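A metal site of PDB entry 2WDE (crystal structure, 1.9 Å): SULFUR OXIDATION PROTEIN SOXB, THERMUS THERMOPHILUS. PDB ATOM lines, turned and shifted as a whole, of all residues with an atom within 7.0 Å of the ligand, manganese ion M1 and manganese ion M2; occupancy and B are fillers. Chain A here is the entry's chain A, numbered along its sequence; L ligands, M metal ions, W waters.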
ATOM      1  N   SER A  35      -4.204  -6.192 -11.043  1.00  0.00           N
ATOM      2  CA  SER A  35      -3.872  -6.872  -9.794  1.00  0.00           C
ATOM      3  C   SER A  35      -2.499  -7.465  -9.912  1.00  0.00           C
ATOM      4  O   SER A  35      -1.977  -7.623 -11.017  1.00  0.00           O
ATOM      5  CB  SER A  35      -4.888  -7.994  -9.531  1.00  0.00           C
ATOM      6  OG  SER A  35      -4.699  -8.570  -8.247  1.00  0.00           O
ATOM      7  N   ASP A  36      -1.905  -7.776  -8.764  1.00  0.00           N
ATOM      8  CA  ASP A  36      -0.611  -8.443  -8.730  1.00  0.00           C
ATOM      9  C   ASP A  36       0.513  -7.739  -9.512  1.00  0.00           C
ATOM     10  O   ASP A  36       1.328  -8.374 -10.204  1.00  0.00           O
ATOM     11  CB  ASP A  36      -0.767  -9.904  -9.156  1.00  0.00           C
ATOM     12  CG  ASP A  36      -1.647 -10.703  -8.182  1.00  0.00           C
ATOM     13  OD1 ASP A  36      -1.120 -11.299  -7.213  1.00  0.00           O
ATOM     14  OD2 ASP A  36      -2.886 -10.722  -8.374  1.00  0.00           O
ATOM     15  N   LEU A  37       0.575  -6.426  -9.368  1.00  0.00           N
ATOM     16  CA  LEU A  37       1.607  -5.640 -10.019  1.00  0.00           C
ATOM     17  C   LEU A  37       2.978  -6.044  -9.472  1.00  0.00           C
ATOM     18  O   LEU A  37       3.970  -6.044 -10.188  1.00  0.00           O
ATOM     19  CB  LEU A  37       1.377  -4.138  -9.786  1.00  0.00           C
ATOM     20  CG  LEU A  37       2.405  -3.160 -10.349  1.00  0.00           C
ATOM     21  CD1 LEU A  37       2.544  -3.238 -11.851  1.00  0.00           C
ATOM     22  CD2 LEU A  37       2.043  -1.737  -9.929  1.00  0.00           C
ATOM     23  N   HIS A  38       3.020  -6.434  -8.200  1.00  0.00           N
ATOM     24  CA  HIS A  38       4.277  -6.831  -7.558  1.00  0.00           C
ATOM     25  C   HIS A  38       5.398  -5.807  -7.774  1.00  0.00           C
ATOM     26  O   HIS A  38       6.511  -6.141  -8.187  1.00  0.00           O
ATOM     27  CB  HIS A  38       4.688  -8.250  -7.997  1.00  0.00           C
ATOM     28  CG  HIS A  38       3.893  -9.325  -7.329  1.00  0.00           C
ATOM     29  ND1 HIS A  38       4.207  -9.815  -6.079  1.00  0.00           N
ATOM     30  CD2 HIS A  38       2.809 -10.020  -7.732  1.00  0.00           C
ATOM     31  CE1 HIS A  38       3.348 -10.751  -5.736  1.00  0.00           C
ATOM     32  NE2 HIS A  38       2.485 -10.903  -6.723  1.00  0.00           N
ATOM     33  N   GLY A 130      -6.197  -5.188  -7.151  1.00  0.00           N
ATOM     34  CA  GLY A 130      -6.385  -6.491  -6.542  1.00  0.00           C
ATOM     35  C   GLY A 130      -5.369  -6.941  -5.508  1.00  0.00           C
ATOM     36  O   GLY A 130      -5.514  -8.022  -4.947  1.00  0.00           O
ATOM     37  N   GLY A 131      -4.343  -6.143  -5.230  1.00  0.00           N
ATOM     38  CA  GLY A 131      -3.362  -6.522  -4.213  1.00  0.00           C
ATOM     39  C   GLY A 131      -2.094  -7.164  -4.765  1.00  0.00           C
ATOM     40  O   GLY A 131      -1.957  -7.344  -5.982  1.00  0.00           O
ATOM     41  N   ASP A 132      -1.160  -7.489  -3.865  1.00  0.00           N
ATOM     42  CA  ASP A 132       0.162  -7.987  -4.263  1.00  0.00           C
ATOM     43  C   ASP A 132       0.756  -6.884  -5.110  1.00  0.00           C
ATOM     44  O   ASP A 132       1.317  -7.104  -6.178  1.00  0.00           O
ATOM     45  CB  ASP A 132       0.088  -9.299  -5.040  1.00  0.00           C
ATOM     46  CG  ASP A 132       0.092 -10.501  -4.127  1.00  0.00           C
ATOM     47  OD1 ASP A 132       0.048 -10.271  -2.890  1.00  0.00           O
ATOM     48  OD2 ASP A 132       0.072 -11.643  -4.616  1.00  0.00           O
ATOM     49  N   THR A 133       0.600  -5.674  -4.591  1.00  0.00           N
ATOM     50  CA  THR A 133       1.053  -4.472  -5.267  1.00  0.00           C
ATOM     51  C   THR A 133       2.344  -3.855  -4.720  1.00  0.00           C
ATOM     52  O   THR A 133       3.198  -3.420  -5.492  1.00  0.00           O
ATOM     53  CB  THR A 133      -0.060  -3.393  -5.172  1.00  0.00           C
ATOM     54  OG1 THR A 133      -1.308  -3.953  -5.590  1.00  0.00           O
ATOM     55  CG2 THR A 133       0.286  -2.180  -6.036  1.00  0.00           C
ATOM     56  N   ASN A 136       7.956  -6.906  -3.709  1.00  0.00           N
ATOM     57  CA  ASN A 136       8.683  -7.685  -4.718  1.00  0.00           C
ATOM     58  C   ASN A 136       9.265  -6.984  -5.941  1.00  0.00           C
ATOM     59  O   ASN A 136       9.091  -7.452  -7.070  1.00  0.00           O
ATOM     60  CB  ASN A 136       7.841  -8.894  -5.111  1.00  0.00           C
ATOM     61  CG  ASN A 136       7.076  -9.467  -3.924  1.00  0.00           C
ATOM     62  OD1 ASN A 136       5.852  -9.390  -3.881  1.00  0.00           O
ATOM     63  ND2 ASN A 136       7.803 -10.003  -2.946  1.00  0.00           N
ATOM     64  N   SER A 162      -5.417  -7.021  -0.232  1.00  0.00           N
ATOM     65  CA  SER A 162      -4.020  -7.376   0.040  1.00  0.00           C
ATOM     66  C   SER A 162      -3.674  -8.845   0.140  1.00  0.00           C
ATOM     67  O   SER A 162      -4.534  -9.731   0.311  1.00  0.00           O
ATOM     68  CB  SER A 162      -3.630  -6.735   1.380  1.00  0.00           C
ATOM     69  OG  SER A 162      -4.231  -7.461   2.453  1.00  0.00           O
ATOM     70  N   HIS A 163      -2.366  -9.088   0.115  1.00  0.00           N
ATOM     71  CA  HIS A 163      -1.776 -10.392   0.348  1.00  0.00           C
ATOM     72  C   HIS A 163      -0.322 -10.184   0.734  1.00  0.00           C
ATOM     73  O   HIS A 163      -0.004 -10.066   1.931  1.00  0.00           O
ATOM     74  CB  HIS A 163      -1.900 -11.346  -0.845  1.00  0.00           C
ATOM     75  CG  HIS A 163      -1.070 -12.587  -0.694  1.00  0.00           C
ATOM     76  ND1 HIS A 163      -0.798 -13.448  -1.735  1.00  0.00           N
ATOM     77  CD2 HIS A 163      -0.434 -13.108   0.385  1.00  0.00           C
ATOM     78  CE1 HIS A 163      -0.017 -14.421  -1.314  1.00  0.00           C
ATOM     79  NE2 HIS A 163       0.195 -14.255  -0.022  1.00  0.00           N
ATOM     80  N   TRP A 164       0.555 -10.075  -0.261  1.00  0.00           N
ATOM     81  CA  TRP A 164       1.996  -9.897  -0.018  1.00  0.00           C
ATOM     82  C   TRP A 164       2.354  -8.588   0.690  1.00  0.00           C
ATOM     83  O   TRP A 164       3.462  -8.434   1.220  1.00  0.00           O
ATOM     84  CB  TRP A 164       2.791 -10.058  -1.326  1.00  0.00           C
ATOM     85  CG  TRP A 164       3.113 -11.506  -1.675  1.00  0.00           C
ATOM     86  CD1 TRP A 164       2.309 -12.396  -2.337  1.00  0.00           C
ATOM     87  CD2 TRP A 164       4.316 -12.209  -1.367  1.00  0.00           C
ATOM     88  NE1 TRP A 164       2.964 -13.603  -2.489  1.00  0.00           N
ATOM     89  CE2 TRP A 164       4.185 -13.513  -1.888  1.00  0.00           C
ATOM     90  CE3 TRP A 164       5.506 -11.860  -0.707  1.00  0.00           C
ATOM     91  CZ2 TRP A 164       5.175 -14.496  -1.719  1.00  0.00           C
ATOM     92  CZ3 TRP A 164       6.504 -12.833  -0.565  1.00  0.00           C
ATOM     93  CH2 TRP A 164       6.323 -14.126  -1.084  1.00  0.00           C
ATOM     94  N   TYR A 219      -6.199 -12.261   0.868  1.00  0.00           N
ATOM     95  CA  TYR A 219      -5.777 -13.666   0.826  1.00  0.00           C
ATOM     96  C   TYR A 219      -5.970 -14.308   2.207  1.00  0.00           C
ATOM     97  O   TYR A 219      -5.463 -13.800   3.206  1.00  0.00           O
ATOM     98  CB  TYR A 219      -4.308 -13.758   0.389  1.00  0.00           C
ATOM     99  CG  TYR A 219      -3.816 -15.151   0.114  1.00  0.00           C
ATOM    100  CD1 TYR A 219      -4.471 -15.977  -0.794  1.00  0.00           C
ATOM    101  CD2 TYR A 219      -2.672 -15.644   0.725  1.00  0.00           C
ATOM    102  CE1 TYR A 219      -4.032 -17.269  -1.045  1.00  0.00           C
ATOM    103  CE2 TYR A 219      -2.211 -16.914   0.463  1.00  0.00           C
ATOM    104  CZ  TYR A 219      -2.884 -17.716  -0.410  1.00  0.00           C
ATOM    105  OH  TYR A 219      -2.410 -18.981  -0.662  1.00  0.00           O
ATOM    106  N   HIS A 226       3.651 -17.081   5.026  1.00  0.00           N
ATOM    107  CA  HIS A 226       4.738 -16.146   5.304  1.00  0.00           C
ATOM    108  C   HIS A 226       5.082 -16.170   6.788  1.00  0.00           C
ATOM    109  O   HIS A 226       4.304 -16.697   7.572  1.00  0.00           O
ATOM    110  CB  HIS A 226       4.294 -14.735   4.913  1.00  0.00           C
ATOM    111  CG  HIS A 226       3.640 -14.682   3.574  1.00  0.00           C
ATOM    112  ND1 HIS A 226       4.362 -14.663   2.396  1.00  0.00           N
ATOM    113  CD2 HIS A 226       2.330 -14.677   3.208  1.00  0.00           C
ATOM    114  CE1 HIS A 226       3.527 -14.660   1.373  1.00  0.00           C
ATOM    115  NE2 HIS A 226       2.286 -14.655   1.832  1.00  0.00           N
ATOM    116  N   HIS A 263      -8.700 -11.429  -3.424  1.00  0.00           N
ATOM    117  CA  HIS A 263      -7.349 -11.964  -3.487  1.00  0.00           C
ATOM    118  C   HIS A 263      -7.385 -13.346  -2.865  1.00  0.00           C
ATOM    119  O   HIS A 263      -6.426 -13.782  -2.229  1.00  0.00           O
ATOM    120  CB  HIS A 263      -6.299 -11.056  -2.828  1.00  0.00           C
ATOM    121  CG  HIS A 263      -4.913 -11.276  -3.333  1.00  0.00           C
ATOM    122  ND1 HIS A 263      -4.264 -10.388  -4.169  1.00  0.00           N
ATOM    123  CD2 HIS A 263      -4.069 -12.336  -3.200  1.00  0.00           C
ATOM    124  CE1 HIS A 263      -3.079 -10.864  -4.488  1.00  0.00           C
ATOM    125  NE2 HIS A 263      -2.923 -12.036  -3.900  1.00  0.00           N
ATOM    126  N   GLY A 285      -7.988 -11.772  -8.152  1.00  0.00           N
ATOM    127  CA  GLY A 285      -6.548 -11.595  -8.129  1.00  0.00           C
ATOM    128  C   GLY A 285      -5.885 -12.881  -7.622  1.00  0.00           C
ATOM    129  O   GLY A 285      -6.519 -13.926  -7.587  1.00  0.00           O
ATOM    130  N   HIS A 286      -4.614 -12.781  -7.223  1.00  0.00           N
ATOM    131  CA  HIS A 286      -3.813 -13.873  -6.644  1.00  0.00           C
ATOM    132  C   HIS A 286      -3.302 -14.957  -7.576  1.00  0.00           C
ATOM    133  O   HIS A 286      -2.127 -15.337  -7.498  1.00  0.00           O
ATOM    134  CB  HIS A 286      -4.497 -14.514  -5.442  1.00  0.00           C
ATOM    135  CG  HIS A 286      -3.663 -15.566  -4.775  1.00  0.00           C
ATOM    136  ND1 HIS A 286      -2.466 -15.276  -4.126  1.00  0.00           N
ATOM    137  CD2 HIS A 286      -3.833 -16.900  -4.647  1.00  0.00           C
ATOM    138  CE1 HIS A 286      -1.937 -16.392  -3.670  1.00  0.00           C
ATOM    139  NE2 HIS A 286      -2.748 -17.395  -3.961  1.00  0.00           N
ATOM    140  N   THR A 287      -4.178 -15.505  -8.416  1.00  0.00           N
ATOM    141  CA  THR A 287      -3.747 -16.576  -9.303  1.00  0.00           C
ATOM    142  C   THR A 287      -3.054 -16.095 -10.582  1.00  0.00           C
ATOM    143  O   THR A 287      -2.576 -16.909 -11.364  1.00  0.00           O
ATOM    144  CB  THR A 287      -4.865 -17.598  -9.575  1.00  0.00           C
ATOM    145  OG1 THR A 287      -6.114 -16.919  -9.711  1.00  0.00           O
ATOM    146  CG2 THR A 287      -4.957 -18.589  -8.390  1.00  0.00           C
ATOM    147  N   HIS A 288      -2.979 -14.774 -10.756  1.00  0.00           N
ATOM    148  CA  HIS A 288      -2.291 -14.185 -11.916  1.00  0.00           C
ATOM    149  C   HIS A 288      -2.913 -14.643 -13.249  1.00  0.00           C
ATOM    150  O   HIS A 288      -2.231 -14.781 -14.257  1.00  0.00           O
ATOM    151  CB  HIS A 288      -0.778 -14.526 -11.878  1.00  0.00           C
ATOM    152  CG  HIS A 288      -0.026 -13.868 -10.760  1.00  0.00           C
ATOM    153  ND1 HIS A 288       1.319 -13.565 -10.845  1.00  0.00           N
ATOM    154  CD2 HIS A 288      -0.418 -13.461  -9.526  1.00  0.00           C
ATOM    155  CE1 HIS A 288       1.719 -13.019  -9.711  1.00  0.00           C
ATOM    156  NE2 HIS A 288       0.687 -12.932  -8.899  1.00  0.00           N
ATOM    157  N   SER A 306      -4.773 -10.575 -13.908  1.00  0.00           N
ATOM    158  CA  SER A 306      -3.481 -10.734 -14.582  1.00  0.00           C
ATOM    159  C   SER A 306      -2.349 -10.411 -13.616  1.00  0.00           C
ATOM    160  O   SER A 306      -2.452 -10.725 -12.426  1.00  0.00           O
ATOM    161  CB  SER A 306      -3.396  -9.858 -15.835  1.00  0.00           C
ATOM    162  OG  SER A 306      -2.271 -10.213 -16.622  1.00  0.00           O
ATOM    163  N   ALA A 307      -1.281  -9.769 -14.097  1.00  0.00           N
ATOM    164  CA  ALA A 307      -0.150  -9.510 -13.222  1.00  0.00           C
ATOM    165  C   ALA A 307       1.001  -8.704 -13.820  1.00  0.00           C
ATOM    166  O   ALA A 307       1.134  -8.583 -15.038  1.00  0.00           O
ATOM    167  CB  ALA A 307       0.391 -10.836 -12.687  1.00  0.00           C
ATOM    168  N   ALA A 403       7.926 -21.763  -5.768  1.00  0.00           N
ATOM    169  CA  ALA A 403       7.087 -21.626  -6.948  1.00  0.00           C
ATOM    170  C   ALA A 403       6.105 -20.474  -6.857  1.00  0.00           C
ATOM    171  O   ALA A 403       4.906 -20.643  -7.093  1.00  0.00           O
ATOM    172  CB  ALA A 403       6.375 -22.940  -7.241  1.00  0.00           C
ATOM    173  N   VAL A 404       6.615 -19.292  -6.511  1.00  0.00           N
ATOM    174  CA  VAL A 404       5.780 -18.090  -6.488  1.00  0.00           C
ATOM    175  C   VAL A 404       5.357 -17.764  -7.930  1.00  0.00           C
ATOM    176  O   VAL A 404       6.004 -18.197  -8.885  1.00  0.00           O
ATOM    177  CB  VAL A 404       6.495 -16.893  -5.804  1.00  0.00           C
ATOM    178  CG1 VAL A 404       6.803 -17.226  -4.341  1.00  0.00           C
ATOM    179  CG2 VAL A 404       7.773 -16.495  -6.564  1.00  0.00           C
ATOM    180  N   ARG A 405       4.258 -17.020  -8.061  1.00  0.00           N
ATOM    181  CA  ARG A 405       3.694 -16.609  -9.345  1.00  0.00           C
ATOM    182  C   ARG A 405       4.284 -15.292  -9.864  1.00  0.00           C
ATOM    183  O   ARG A 405       4.073 -14.925 -11.010  1.00  0.00           O
ATOM    184  CB  ARG A 405       2.182 -16.396  -9.171  1.00  0.00           C
ATOM    185  CG  ARG A 405       1.410 -17.675  -8.914  1.00  0.00           C
ATOM    186  CD  ARG A 405      -0.098 -17.456  -9.084  1.00  0.00           C
ATOM    187  NE  ARG A 405      -0.814 -18.706  -8.859  1.00  0.00           N
ATOM    188  CZ  ARG A 405      -1.139 -19.180  -7.659  1.00  0.00           C
ATOM    189  NH1 ARG A 405      -0.869 -18.470  -6.570  1.00  0.00           N
ATOM    190  NH2 ARG A 405      -1.746 -20.339  -7.530  1.00  0.00           N
ATOM    191  N   TRP A 406       4.942 -14.556  -8.978  1.00  0.00           N
ATOM    192  CA  TRP A 406       5.553 -13.310  -9.376  1.00  0.00           C
ATOM    193  C   TRP A 406       6.958 -13.513  -9.959  1.00  0.00           C
ATOM    194  O   TRP A 406       7.617 -14.527  -9.700  1.00  0.00           O
ATOM    195  CB  TRP A 406       5.579 -12.294  -8.221  1.00  0.00           C
ATOM    196  CG  TRP A 406       6.046 -12.812  -6.882  1.00  0.00           C
ATOM    197  CD1 TRP A 406       5.272 -13.337  -5.894  1.00  0.00           C
ATOM    198  CD2 TRP A 406       7.352 -12.621  -6.316  1.00  0.00           C
ATOM    199  NE1 TRP A 406       6.031 -13.569  -4.772  1.00  0.00           N
ATOM    200  CE2 TRP A 406       7.311 -13.142  -5.005  1.00  0.00           C
ATOM    201  CE3 TRP A 406       8.574 -12.169  -6.826  1.00  0.00           C
ATOM    202  CZ2 TRP A 406       8.444 -13.177  -4.182  1.00  0.00           C
ATOM    203  CZ3 TRP A 406       9.694 -12.194  -5.999  1.00  0.00           C
ATOM    204  CH2 TRP A 406       9.621 -12.704  -4.701  1.00  0.00           C
HETATM  205  S1  LIG L   1       1.454 -15.092  -5.258  1.00  0.00           S
HETATM  206  O1  LIG L   1       0.797 -14.695  -4.029  1.00  0.00           O
HETATM  207  O2  LIG L   1       2.010 -13.962  -6.002  1.00  0.00           O
HETATM  208  O3  LIG L   1       0.615 -15.952  -6.085  1.00  0.00           O
HETATM  209  S2  LIG L   1       3.053 -16.220  -4.710  1.00  0.00           S
HETATM  210 MN    MN M   1       0.710 -12.245  -6.742  1.00  0.00          MN
HETATM  211 MN    MN M   2      -1.160 -13.369  -3.924  1.00  0.00          MN
HETATM  212  O   HOH W   1      -0.588 -13.607  -6.164  1.00  0.00           O
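NE1 of Trp 164 lies close to S2 of the ligand. The backbone NH (N) of Arg 405 lies close to a sulfur (S2) of the ligand (3.6 Å). O3 of the ligand is in salt-bridge range of NH1 of Arg 405 (3.0 Å).
The side-chain carboxylate (OD2) of Asp 36 is in hydrogen-bond range of the backbone NH (N) of His 286 (2.9 Å). The backbone carbonyl oxygen of Gly 131 lies within hydrogen-bond range of the backbone NH of Asp 36. OG of Ser 35 sits at hydrogen-bond distance from OD2 of Asp 36 (2.8 Å). NE2 of His 163 sits at hydrogen-bond distance from NE2 of His 226, at 2.8 Å. The side-chain amide oxygen (OD1) of Asn 136 lies within hydrogen-bond range of a ring nitrogen (ND1) of His 38 (2.8 Å). The backbone carbonyl oxygen of Asp 132 is in hydrogen-bond range of the backbone NH of Leu 37, at 3.3 Å. A ring nitrogen (ND1) of His 288 lies within hydrogen-bond range of the backbone carbonyl oxygen (O) of Arg 405, at 3.1 Å. NE2 of His 286 sits at hydrogen-bond distance from NH1 of Arg 405 (3.4 Å).
Val 404 touches the ligand. Trp 406 touches the ligand. The nearest printed residue that does not touch the ligand is Asp 36 (4.3 Å).
Within 4 Å of manganese ion M1: Asp 36, His 38, Asp 132 and His 288.
Merely in contact with manganese ion M2: Trp 164 (3.9 Å). Six residues have an atom within 4 Å of manganese ion M2: Asp 36, Asp 132, His 163, Trp 164, His 263 and His 286. The nearest printed residue that does not touch manganese ion M2 is Tyr 219 (5.2 Å).
Manganese ion M1 is bound by water W1 (2.0 Å), the side-chain carboxylate of Asp 36 (2.1 Å), a ring nitrogen (NE2) of His 38 (2.2 Å), a ring nitrogen (NE2) of His 288 (2.3 Å), an oxygen (O2) of the ligand (2.3 Å) and the side-chain carboxylate of Asp 132 (2.3 Å).
A ring nitrogen (NE2) of His 263 binds manganese ion M2 (2.2 Å). Manganese ion M2 is bound by a ring nitrogen (ND1) of His 163. The side-chain carboxylate (OD2) of Asp 132 is bound to manganese ion M2 (2.2 Å). A ring nitrogen (ND1) of His 286 is bound to manganese ion M2 (2.3 Å). Water W1 is bound to manganese ion M2 (2.3 Å). O1 of the ligand is bound to manganese ion M2, at 2.4 Å.
Water W1 lies within hydrogen-bond range of O3 of the ligand and O of His 286.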
